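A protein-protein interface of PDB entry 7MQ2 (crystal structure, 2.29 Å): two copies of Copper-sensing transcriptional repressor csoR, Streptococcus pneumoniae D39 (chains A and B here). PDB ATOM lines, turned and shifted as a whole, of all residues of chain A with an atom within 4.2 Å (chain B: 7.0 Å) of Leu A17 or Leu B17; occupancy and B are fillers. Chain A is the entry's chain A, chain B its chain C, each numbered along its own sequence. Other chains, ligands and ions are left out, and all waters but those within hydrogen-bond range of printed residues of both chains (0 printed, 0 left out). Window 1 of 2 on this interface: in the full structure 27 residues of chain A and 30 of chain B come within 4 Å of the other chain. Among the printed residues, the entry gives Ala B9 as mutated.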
ATOM      1  N   LEU A  10      16.670  15.196 -14.436  1.00  0.00           N
ATOM      2  CA  LEU A  10      16.321  14.727 -13.100  1.00  0.00           C
ATOM      3  C   LEU A  10      14.938  14.108 -13.056  1.00  0.00           C
ATOM      4  O   LEU A  10      14.682  13.234 -12.216  1.00  0.00           O
ATOM      5  CB  LEU A  10      16.411  15.872 -12.100  1.00  0.00           C
ATOM      6  CG  LEU A  10      17.859  16.266 -11.777  1.00  0.00           C
ATOM      7  CD1 LEU A  10      17.839  17.313 -10.703  1.00  0.00           C
ATOM      8  CD2 LEU A  10      18.765  15.073 -11.455  1.00  0.00           C
ATOM      9  N   SER A  13      15.670  10.548 -14.041  1.00  0.00           N
ATOM     10  CA  SER A  13      16.178   9.796 -12.880  1.00  0.00           C
ATOM     11  C   SER A  13      15.075   9.462 -11.868  1.00  0.00           C
ATOM     12  O   SER A  13      15.052   8.351 -11.314  1.00  0.00           O
ATOM     13  CB  SER A  13      17.281  10.582 -12.173  1.00  0.00           C
ATOM     14  OG  SER A  13      18.260  11.086 -13.077  1.00  0.00           O
ATOM     15  N   GLU A  14      14.127  10.401 -11.665  1.00  0.00           N
ATOM     16  CA  GLU A  14      12.979  10.204 -10.770  1.00  0.00           C
ATOM     17  C   GLU A  14      12.054   9.088 -11.270  1.00  0.00           C
ATOM     18  O   GLU A  14      11.681   8.182 -10.507  1.00  0.00           O
ATOM     19  CB  GLU A  14      12.203  11.542 -10.657  1.00  0.00           C
ATOM     20  CG  GLU A  14      10.899  11.499  -9.852  1.00  0.00           C
ATOM     21  CD  GLU A  14       9.916  12.657 -10.155  1.00  0.00           C
ATOM     22  OE1 GLU A  14       8.718  12.579  -9.752  1.00  0.00           O
ATOM     23  OE2 GLU A  14      10.330  13.657 -10.777  1.00  0.00           O
ATOM     24  N   GLY A  15      11.748   9.113 -12.573  1.00  0.00           N
ATOM     25  CA  GLY A  15      10.970   8.039 -13.199  1.00  0.00           C
ATOM     26  C   GLY A  15      11.647   6.678 -13.167  1.00  0.00           C
ATOM     27  O   GLY A  15      10.984   5.664 -12.903  1.00  0.00           O
ATOM     28  N   GLN A  16      12.988   6.651 -13.349  1.00  0.00           N
ATOM     29  CA  GLN A  16      13.743   5.398 -13.249  1.00  0.00           C
ATOM     30  C   GLN A  16      13.727   4.826 -11.839  1.00  0.00           C
ATOM     31  O   GLN A  16      13.668   3.598 -11.673  1.00  0.00           O
ATOM     32  CB  GLN A  16      15.212   5.574 -13.642  1.00  0.00           C
ATOM     33  CG  GLN A  16      15.602   5.886 -15.079  1.00  0.00           C
ATOM     34  CD  GLN A  16      17.143   5.861 -15.232  1.00  0.00           C
ATOM     35  OE1 GLN A  16      17.755   4.779 -15.216  1.00  0.00           O
ATOM     36  NE2 GLN A  16      17.776   7.053 -15.151  1.00  0.00           N
ATOM     37  N   LEU A  17      13.776   5.697 -10.811  1.00  0.00           N
ATOM     38  CA  LEU A  17      13.620   5.200  -9.441  1.00  0.00           C
ATOM     39  C   LEU A  17      12.222   4.643  -9.187  1.00  0.00           C
ATOM     40  O   LEU A  17      12.079   3.674  -8.429  1.00  0.00           O
ATOM     41  CB  LEU A  17      13.935   6.299  -8.435  1.00  0.00           C
ATOM     42  CG  LEU A  17      15.422   6.721  -8.268  1.00  0.00           C
ATOM     43  CD1 LEU A  17      15.494   7.848  -7.269  1.00  0.00           C
ATOM     44  CD2 LEU A  17      16.251   5.517  -7.776  1.00  0.00           C
ATOM     45  N   ARG A  18      11.209   5.207  -9.844  1.00  0.00           N
ATOM     46  CA  ARG A  18       9.855   4.610  -9.765  1.00  0.00           C
ATOM     47  C   ARG A  18       9.807   3.228 -10.437  1.00  0.00           C
ATOM     48  O   ARG A  18       9.211   2.285  -9.879  1.00  0.00           O
ATOM     49  CB  ARG A  18       8.806   5.555 -10.376  1.00  0.00           C
ATOM     50  CG  ARG A  18       7.960   6.296  -9.315  1.00  0.00           C
ATOM     51  CD  ARG A  18       6.707   7.026  -9.898  1.00  0.00           C
ATOM     52  NE  ARG A  18       7.069   7.717 -11.127  1.00  0.00           N
ATOM     53  CZ  ARG A  18       7.622   8.922 -11.174  1.00  0.00           C
ATOM     54  NH1 ARG A  18       7.770   9.632 -10.032  1.00  0.00           N
ATOM     55  NH2 ARG A  18       7.965   9.435 -12.373  1.00  0.00           N
ATOM     56  N   GLY A  19      10.525   3.096 -11.569  1.00  0.00           N
ATOM     57  CA  GLY A  19      10.676   1.815 -12.241  1.00  0.00           C
ATOM     58  C   GLY A  19      11.364   0.770 -11.384  1.00  0.00           C
ATOM     59  O   GLY A  19      10.903  -0.370 -11.313  1.00  0.00           O
ATOM     60  N   ILE A  20      12.361   1.196 -10.596  1.00  0.00           N
ATOM     61  CA  ILE A  20      13.115   0.247  -9.775  1.00  0.00           C
ATOM     62  C   ILE A  20      12.291  -0.239  -8.590  1.00  0.00           C
ATOM     63  O   ILE A  20      12.272  -1.457  -8.286  1.00  0.00           O
ATOM     64  CB  ILE A  20      14.434   0.899  -9.338  1.00  0.00           C
ATOM     65  CG1 ILE A  20      15.324   0.994 -10.564  1.00  0.00           C
ATOM     66  CG2 ILE A  20      15.123   0.103  -8.263  1.00  0.00           C
ATOM     67  CD1 ILE A  20      16.495   1.910 -10.396  1.00  0.00           C
ATOM     68  N   GLN A  21      11.558   0.696  -7.949  1.00  0.00           N
ATOM     69  CA  GLN A  21      10.525   0.357  -6.956  1.00  0.00           C
ATOM     70  C   GLN A  21       9.516  -0.678  -7.464  1.00  0.00           C
ATOM     71  O   GLN A  21       9.263  -1.680  -6.774  1.00  0.00           O
ATOM     72  CB  GLN A  21       9.770   1.619  -6.526  1.00  0.00           C
ATOM     73  CG  GLN A  21      10.577   2.637  -5.738  1.00  0.00           C
ATOM     74  CD  GLN A  21       9.923   4.018  -5.833  1.00  0.00           C
ATOM     75  OE1 GLN A  21       8.694   4.123  -5.753  1.00  0.00           O
ATOM     76  NE2 GLN A  21      10.731   5.074  -6.025  1.00  0.00           N
ATOM     77  N   VAL A  40      20.924   4.910 -12.470  1.00  0.00           N
ATOM     78  CA  VAL A  40      20.374   6.106 -11.808  1.00  0.00           C
ATOM     79  C   VAL A  40      21.484   6.935 -11.190  1.00  0.00           C
ATOM     80  O   VAL A  40      21.561   8.154 -11.415  1.00  0.00           O
ATOM     81  CB  VAL A  40      19.343   5.715 -10.730  1.00  0.00           C
ATOM     82  CG1 VAL A  40      18.962   6.953  -9.869  1.00  0.00           C
ATOM     83  CG2 VAL A  40      18.132   5.129 -11.376  1.00  0.00           C
ATOM     84  N   VAL A  44      22.498  10.814 -12.158  1.00  0.00           N
ATOM     85  CA  VAL A  44      22.599  11.869 -11.143  1.00  0.00           C
ATOM     86  C   VAL A  44      23.997  12.494 -11.165  1.00  0.00           C
ATOM     87  O   VAL A  44      24.133  13.729 -11.189  1.00  0.00           O
ATOM     88  CB  VAL A  44      22.241  11.314  -9.739  1.00  0.00           C
ATOM     89  CG1 VAL A  44      22.618  12.319  -8.633  1.00  0.00           C
ATOM     90  CG2 VAL A  44      20.746  10.958  -9.628  1.00  0.00           C
ATOM     91  N   ILE B   7      12.081  -0.095  -1.106  1.00  0.00           N
ATOM     92  CA  ILE B   7      11.025   0.745  -1.705  1.00  0.00           C
ATOM     93  C   ILE B   7      10.996   2.128  -1.052  1.00  0.00           C
ATOM     94  O   ILE B   7      11.059   3.155  -1.749  1.00  0.00           O
ATOM     95  CB  ILE B   7       9.628   0.108  -1.536  1.00  0.00           C
ATOM     96  CG1 ILE B   7       9.466  -1.294  -2.139  1.00  0.00           C
ATOM     97  CG2 ILE B   7       8.569   1.033  -2.174  1.00  0.00           C
ATOM     98  CD1 ILE B   7       9.606  -1.323  -3.519  1.00  0.00           C
ATOM     99  N   ALA B   9      13.331   3.638   0.855  1.00  0.00           N
ATOM    100  CA  ALA B   9      14.573   4.389   0.608  1.00  0.00           C
ATOM    101  C   ALA B   9      14.642   4.988  -0.801  1.00  0.00           C
ATOM    102  O   ALA B   9      15.001   6.176  -0.961  1.00  0.00           O
ATOM    103  CB  ALA B   9      15.769   3.491   0.871  1.00  0.00           C
ATOM    104  N   LEU B  10      14.134   4.253  -1.813  1.00  0.00           N
ATOM    105  CA  LEU B  10      14.083   4.855  -3.142  1.00  0.00           C
ATOM    106  C   LEU B  10      12.942   5.857  -3.321  1.00  0.00           C
ATOM    107  O   LEU B  10      13.089   6.792  -4.118  1.00  0.00           O
ATOM    108  CB  LEU B  10      13.997   3.766  -4.206  1.00  0.00           C
ATOM    109  CG  LEU B  10      15.249   2.870  -4.126  1.00  0.00           C
ATOM    110  CD1 LEU B  10      14.976   1.634  -4.889  1.00  0.00           C
ATOM    111  CD2 LEU B  10      16.535   3.531  -4.554  1.00  0.00           C
ATOM    112  N   LYS B  11      11.824   5.689  -2.606  1.00  0.00           N
ATOM    113  CA  LYS B  11      10.800   6.745  -2.521  1.00  0.00           C
ATOM    114  C   LYS B  11      11.357   8.052  -1.926  1.00  0.00           C
ATOM    115  O   LYS B  11      11.088   9.144  -2.458  1.00  0.00           O
ATOM    116  CB  LYS B  11       9.604   6.255  -1.698  1.00  0.00           C
ATOM    117  CG  LYS B  11       8.659   5.338  -2.471  1.00  0.00           C
ATOM    118  CD  LYS B  11       7.678   4.649  -1.534  1.00  0.00           C
ATOM    119  CE  LYS B  11       6.452   4.099  -2.285  1.00  0.00           C
ATOM    120  NZ  LYS B  11       5.837   5.128  -3.189  1.00  0.00           N
ATOM    121  N   ARG B  12      12.202   7.938  -0.887  1.00  0.00           N
ATOM    122  CA  ARG B  12      12.890   9.114  -0.317  1.00  0.00           C
ATOM    123  C   ARG B  12      13.814   9.775  -1.336  1.00  0.00           C
ATOM    124  O   ARG B  12      13.658  10.978  -1.572  1.00  0.00           O
ATOM    125  CB  ARG B  12      13.626   8.749   0.982  1.00  0.00           C
ATOM    126  CG  ARG B  12      12.655   8.161   2.018  1.00  0.00           C
ATOM    127  CD  ARG B  12      13.001   8.245   3.503  1.00  0.00           C
ATOM    128  NE  ARG B  12      11.799   7.979   4.311  1.00  0.00           N
ATOM    129  CZ  ARG B  12      11.715   7.109   5.321  1.00  0.00           C
ATOM    130  NH1 ARG B  12      12.758   6.357   5.650  1.00  0.00           N
ATOM    131  NH2 ARG B  12      10.566   6.949   5.973  1.00  0.00           N
ATOM    132  N   SER B  13      14.566   8.973  -2.125  1.00  0.00           N
ATOM    133  CA  SER B  13      15.466   9.554  -3.145  1.00  0.00           C
ATOM    134  C   SER B  13      14.707  10.170  -4.308  1.00  0.00           C
ATOM    135  O   SER B  13      15.105  11.226  -4.817  1.00  0.00           O
ATOM    136  CB  SER B  13      16.423   8.508  -3.699  1.00  0.00           C
ATOM    137  OG  SER B  13      16.939   7.751  -2.636  1.00  0.00           O
ATOM    138  N   GLU B  14      13.596   9.524  -4.701  1.00  0.00           N
ATOM    139  CA  GLU B  14      12.685  10.005  -5.745  1.00  0.00           C
ATOM    140  C   GLU B  14      12.131  11.387  -5.418  1.00  0.00           C
ATOM    141  O   GLU B  14      12.243  12.332  -6.224  1.00  0.00           O
ATOM    142  CB  GLU B  14      11.534   8.991  -5.872  1.00  0.00           C
ATOM    143  CG  GLU B  14      10.631   9.196  -7.040  1.00  0.00           C
ATOM    144  CD  GLU B  14       9.264   8.511  -6.888  1.00  0.00           C
ATOM    145  OE1 GLU B  14       8.259   9.078  -7.415  1.00  0.00           O
ATOM    146  OE2 GLU B  14       9.188   7.422  -6.255  1.00  0.00           O
ATOM    147  N   GLY B  15      11.635  11.536  -4.184  1.00  0.00           N
ATOM    148  CA  GLY B  15      11.219  12.835  -3.694  1.00  0.00           C
ATOM    149  C   GLY B  15      12.341  13.856  -3.511  1.00  0.00           C
ATOM    150  O   GLY B  15      12.108  15.055  -3.723  1.00  0.00           O
ATOM    151  N   GLN B  16      13.554  13.416  -3.115  1.00  0.00           N
ATOM    152  CA  GLN B  16      14.692  14.355  -3.121  1.00  0.00           C
ATOM    153  C   GLN B  16      15.024  14.854  -4.518  1.00  0.00           C
ATOM    154  O   GLN B  16      15.334  16.035  -4.667  1.00  0.00           O
ATOM    155  CB  GLN B  16      15.988  13.810  -2.504  1.00  0.00           C
ATOM    156  CG  GLN B  16      16.059  13.059  -1.152  1.00  0.00           C
ATOM    157  CD  GLN B  16      17.393  12.248  -0.992  1.00  0.00           C
ATOM    158  OE1 GLN B  16      17.413  10.990  -0.835  1.00  0.00           O
ATOM    159  NE2 GLN B  16      18.505  12.991  -0.939  1.00  0.00           N
ATOM    160  N   LEU B  17      14.852  14.017  -5.565  1.00  0.00           N
ATOM    161  CA  LEU B  17      15.025  14.533  -6.935  1.00  0.00           C
ATOM    162  C   LEU B  17      13.915  15.515  -7.335  1.00  0.00           C
ATOM    163  O   LEU B  17      14.189  16.475  -8.073  1.00  0.00           O
ATOM    164  CB  LEU B  17      15.110  13.393  -7.956  1.00  0.00           C
ATOM    165  CG  LEU B  17      16.388  12.545  -7.835  1.00  0.00           C
ATOM    166  CD1 LEU B  17      16.245  11.246  -8.629  1.00  0.00           C
ATOM    167  CD2 LEU B  17      17.668  13.332  -8.304  1.00  0.00           C
ATOM    168  N   ARG B  18      12.696  15.349  -6.804  1.00  0.00           N
ATOM    169  CA  ARG B  18      11.682  16.399  -7.023  1.00  0.00           C
ATOM    170  C   ARG B  18      12.037  17.716  -6.320  1.00  0.00           C
ATOM    171  O   ARG B  18      11.896  18.797  -6.929  1.00  0.00           O
ATOM    172  CB  ARG B  18      10.297  15.928  -6.573  1.00  0.00           C
ATOM    173  CG  ARG B  18       9.626  15.075  -7.618  1.00  0.00           C
ATOM    174  CD  ARG B  18       8.170  14.793  -7.285  1.00  0.00           C
ATOM    175  NE  ARG B  18       8.016  13.936  -6.122  1.00  0.00           N
ATOM    176  CZ  ARG B  18       7.978  12.606  -6.174  1.00  0.00           C
ATOM    177  NH1 ARG B  18       8.152  11.949  -7.327  1.00  0.00           N
ATOM    178  NH2 ARG B  18       7.813  11.931  -5.052  1.00  0.00           N
ATOM    179  N   GLY B  19      12.552  17.620  -5.077  1.00  0.00           N
ATOM    180  CA  GLY B  19      13.050  18.790  -4.357  1.00  0.00           C
ATOM    181  C   GLY B  19      14.176  19.539  -5.065  1.00  0.00           C
ATOM    182  O   GLY B  19      14.149  20.777  -5.137  1.00  0.00           O
ATOM    183  N   ILE B  20      15.097  18.787  -5.694  1.00  0.00           N
ATOM    184  CA  ILE B  20      16.218  19.414  -6.409  1.00  0.00           C
ATOM    185  C   ILE B  20      15.744  20.071  -7.701  1.00  0.00           C
ATOM    186  O   ILE B  20      16.245  21.162  -8.058  1.00  0.00           O
ATOM    187  CB  ILE B  20      17.347  18.394  -6.667  1.00  0.00           C
ATOM    188  CG1 ILE B  20      17.880  17.905  -5.355  1.00  0.00           C
ATOM    189  CG2 ILE B  20      18.558  18.976  -7.441  1.00  0.00           C
ATOM    190  CD1 ILE B  20      18.745  16.695  -5.521  1.00  0.00           C
ATOM    191  N   GLN B  21      14.736  19.474  -8.379  1.00  0.00           N
ATOM    192  CA  GLN B  21      14.079  20.172  -9.502  1.00  0.00           C
ATOM    193  C   GLN B  21      13.448  21.501  -9.068  1.00  0.00           C
ATOM    194  O   GLN B  21      13.572  22.505  -9.783  1.00  0.00           O
ATOM    195  CB  GLN B  21      13.014  19.292 -10.161  1.00  0.00           C
ATOM    196  CG  GLN B  21      13.487  17.999 -10.875  1.00  0.00           C
ATOM    197  CD  GLN B  21      12.340  16.980 -11.053  1.00  0.00           C
ATOM    198  OE1 GLN B  21      11.243  17.369 -11.425  1.00  0.00           O
ATOM    199  NE2 GLN B  21      12.587  15.692 -10.762  1.00  0.00           N
ATOM    200  N   LYS B  22      12.887  21.547  -7.850  1.00  0.00           N
ATOM    201  CA  LYS B  22      12.298  22.799  -7.358  1.00  0.00           C
ATOM    202  C   LYS B  22      13.372  23.841  -7.041  1.00  0.00           C
ATOM    203  O   LYS B  22      13.197  25.023  -7.353  1.00  0.00           O
ATOM    204  CB  LYS B  22      11.431  22.541  -6.126  1.00  0.00           C
ATOM    205  CG  LYS B  22       9.974  22.262  -6.419  1.00  0.00           C
ATOM    206  CD  LYS B  22       9.317  21.704  -5.166  1.00  0.00           C
ATOM    207  CE  LYS B  22       7.885  21.290  -5.413  1.00  0.00           C
ATOM    208  NZ  LYS B  22       7.402  20.409  -4.308  1.00  0.00           N
ATOM    209  N   GLN B  36      22.885  18.467  -2.560  1.00  0.00           N
ATOM    210  CA  GLN B  36      21.660  17.669  -2.500  1.00  0.00           C
ATOM    211  C   GLN B  36      21.675  16.493  -3.484  1.00  0.00           C
ATOM    212  O   GLN B  36      21.289  15.377  -3.116  1.00  0.00           O
ATOM    213  CB  GLN B  36      20.442  18.564  -2.750  1.00  0.00           C
ATOM    214  CG  GLN B  36      20.202  19.620  -1.711  1.00  0.00           C
ATOM    215  CD  GLN B  36      19.272  19.182  -0.642  1.00  0.00           C
ATOM    216  OE1 GLN B  36      19.594  18.280   0.128  1.00  0.00           O
ATOM    217  NE2 GLN B  36      18.101  19.818  -0.571  1.00  0.00           N
ATOM    218  N   LEU B  37      22.144  16.715  -4.720  1.00  0.00           N
ATOM    219  CA  LEU B  37      22.340  15.620  -5.684  1.00  0.00           C
ATOM    220  C   LEU B  37      23.367  14.584  -5.221  1.00  0.00           C
ATOM    221  O   LEU B  37      23.218  13.383  -5.493  1.00  0.00           O
ATOM    222  CB  LEU B  37      22.781  16.207  -6.995  1.00  0.00           C
ATOM    223  CG  LEU B  37      21.753  16.902  -7.843  1.00  0.00           C
ATOM    224  CD1 LEU B  37      22.423  17.807  -8.828  1.00  0.00           C
ATOM    225  CD2 LEU B  37      20.945  15.837  -8.531  1.00  0.00           C
ATOM    226  N   VAL B  40      21.589  12.423  -2.955  1.00  0.00           N
ATOM    227  CA  VAL B  40      20.727  11.489  -3.696  1.00  0.00           C
ATOM    228  C   VAL B  40      21.545  10.313  -4.199  1.00  0.00           C
ATOM    229  O   VAL B  40      21.172   9.148  -3.965  1.00  0.00           O
ATOM    230  CB  VAL B  40      20.012  12.181  -4.879  1.00  0.00           C
ATOM    231  CG1 VAL B  40      19.217  11.199  -5.660  1.00  0.00           C
ATOM    232  CG2 VAL B  40      19.082  13.178  -4.370  1.00  0.00           C
ATOM    233  N   ARG B  41      22.720  10.626  -4.784  1.00  0.00           N
ATOM    234  CA  ARG B  41      23.667   9.623  -5.292  1.00  0.00           C
ATOM    235  C   ARG B  41      24.134   8.669  -4.195  1.00  0.00           C
ATOM    236  O   ARG B  41      24.033   7.442  -4.361  1.00  0.00           O
ATOM    237  CB  ARG B  41      24.866  10.312  -5.966  1.00  0.00           C
ATOM    238  CG  ARG B  41      25.876   9.251  -6.330  1.00  0.00           C
ATOM    239  CD  ARG B  41      27.162   9.682  -6.899  1.00  0.00           C
ATOM    240  NE  ARG B  41      27.830  10.827  -6.276  1.00  0.00           N
ATOM    241  CZ  ARG B  41      28.473  10.823  -5.112  1.00  0.00           C
ATOM    242  NH1 ARG B  41      28.529   9.729  -4.354  1.00  0.00           N
ATOM    243  NH2 ARG B  41      29.060  11.943  -4.699  1.00  0.00           N
ATOM    244  N   SER B  43      22.426   8.029  -1.339  1.00  0.00           N
ATOM    245  CA  SER B  43      21.364   7.174  -0.828  1.00  0.00           C
ATOM    246  C   SER B  43      21.039   6.048  -1.820  1.00  0.00           C
ATOM    247  O   SER B  43      20.802   4.912  -1.385  1.00  0.00           O
ATOM    248  CB  SER B  43      20.140   8.030  -0.447  1.00  0.00           C
ATOM    249  OG  SER B  43      19.437   8.533  -1.574  1.00  0.00           O
ATOM    250  N   VAL B  44      21.191   6.317  -3.121  1.00  0.00           N
ATOM    251  CA  VAL B  44      21.128   5.277  -4.169  1.00  0.00           C
ATOM    252  C   VAL B  44      22.248   4.233  -3.980  1.00  0.00           C
ATOM    253  O   VAL B  44      21.985   3.014  -3.994  1.00  0.00           O
ATOM    254  CB  VAL B  44      21.188   5.926  -5.574  1.00  0.00           C
ATOM    255  CG1 VAL B  44      21.358   4.859  -6.707  1.00  0.00           C
ATOM    256  CG2 VAL B  44      19.956   6.732  -5.878  1.00  0.00           C
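The side-chain carboxylate of Glu A14 lies within salt-bridge range of the guanidinium group of Arg B18 (2.6 Å).
The side-chain carboxylate (OE2) of Glu A14 sits at hydrogen-bond distance from the side-chain amide nitrogen (NE2) of Gln B21 (3.0 Å).
The guanidinium group of Arg A18 lies within salt-bridge range of the side-chain carboxylate of Glu B14, 2.7 Å away.
The backbone carbonyl oxygen of Leu B10 is in hydrogen-bond range of the side-chain amide nitrogen of Gln A21, at 3.5 Å.
The side-chain amide nitrogen of Gln A21 sits at hydrogen-bond distance from the side-chain carboxylate of Glu B14.
OE1 of Glu A14 is in salt-bridge range of NH1 of Arg A18.
O of Leu A17 lies within hydrogen-bond range of NE2 of Gln A21 (3.1 Å).
OG of Ser B13 sits at hydrogen-bond distance from O of Ala B9 (3.0 Å).
OG of Ser B43 lies within hydrogen-bond range of OG of Ser B13, at 2.8 Å.
OE1 of Glu B14 lies within salt-bridge range of NH1 of Arg B18 (2.9 Å).
O of Leu B17 is in hydrogen-bond range of NE2 of Gln B21, 3.2 Å away.
Among the printed residues, merely in contact across the chains: Gln A21 with Ile B7 (3.3 Å), Val A44 with Leu B37 (3.4 Å), Gln A21 with Lys B11 (3.5 Å), Leu A10 with Gln B21 (3.5 Å), Arg A18 with Arg B18 (3.6 Å), Leu A17 with Glu B14 (3.6 Å), Glu A14 with Glu B14 (3.6 Å), Ile A20 with Leu B10 (3.7 Å), Leu A10 with Leu B37 (3.7 Å), Leu A10 with Ile B20 (3.7 Å), Leu A17 with Leu B17 (3.7 Å), Leu A17 with Ser B13 (3.7 Å), Ser A13 with Leu B17 (3.8 Å), Leu A10 with Leu B17 (3.8 Å), Leu A17 with Leu B10 (3.8 Å) and Glu A14 with Leu B17 (3.8 Å).
Of chain B, only Leu B10 (3.8 Å), Ser B13 (3.7 Å), Glu B14 (3.6 Å) and Leu B17 (3.7 Å) come within 4 Å of Leu A17.
Leu B17 touches just these residues of chain A: Leu A10 (3.8 Å), Ser A13 (3.8 Å), Glu A14 (3.8 Å) and Leu A17 (3.7 Å).
Of the printed residues of chain A, Ser B13 touches Leu A17 (3.7 Å).
Of the printed residues of chain A, Arg B18 touches Glu A14 (2.6 Å) and Arg A18 (3.6 Å).
Gln A16 touches none of the printed residues of chain B.
Gln B36 touches none of the printed residues of chain A.
The nearest residue of chain A that does not touch Leu B17 is Val A44 (4.1 Å).
Of the 12 printed residues of chain A, 8 touch a printed residue of chain B.
Printed residues of chain A that touch a printed residue of chain B: Leu A10, Ser A13, Glu A14, Leu A17, Arg A18, Ile A20, Gln A21 and Val A44.
Hydrophobic or aromatic side chains of chain A within 4 Å of the printed part of chain B: Leu A10, Leu A17, Ile A20 and Val A44.
Of the 21 printed residues of chain B, 10 touch a printed residue of chain A.
Hydrophobic or aromatic side chains of chain B within 4 Å of the printed part of chain A: Ile B7, Leu B10, Leu B17, Ile B20 and Leu B37.
Along chain B the printed residues that touch a printed residue of chain A span positions 7 to 37.
Ser A13 touches Leu B17, and with the chains exchanged Leu A17 touches Ser B13.
Glu B14 touches its own counterpart, Glu A14.
Leu A17 touches its own counterpart, Leu B17.
Arg B18 touches its own counterpart, Arg A18.
Positions printed for both chains: 10, 13, 14, 15, 16, 17, 18, 19, 20, 21, 40 and 44.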
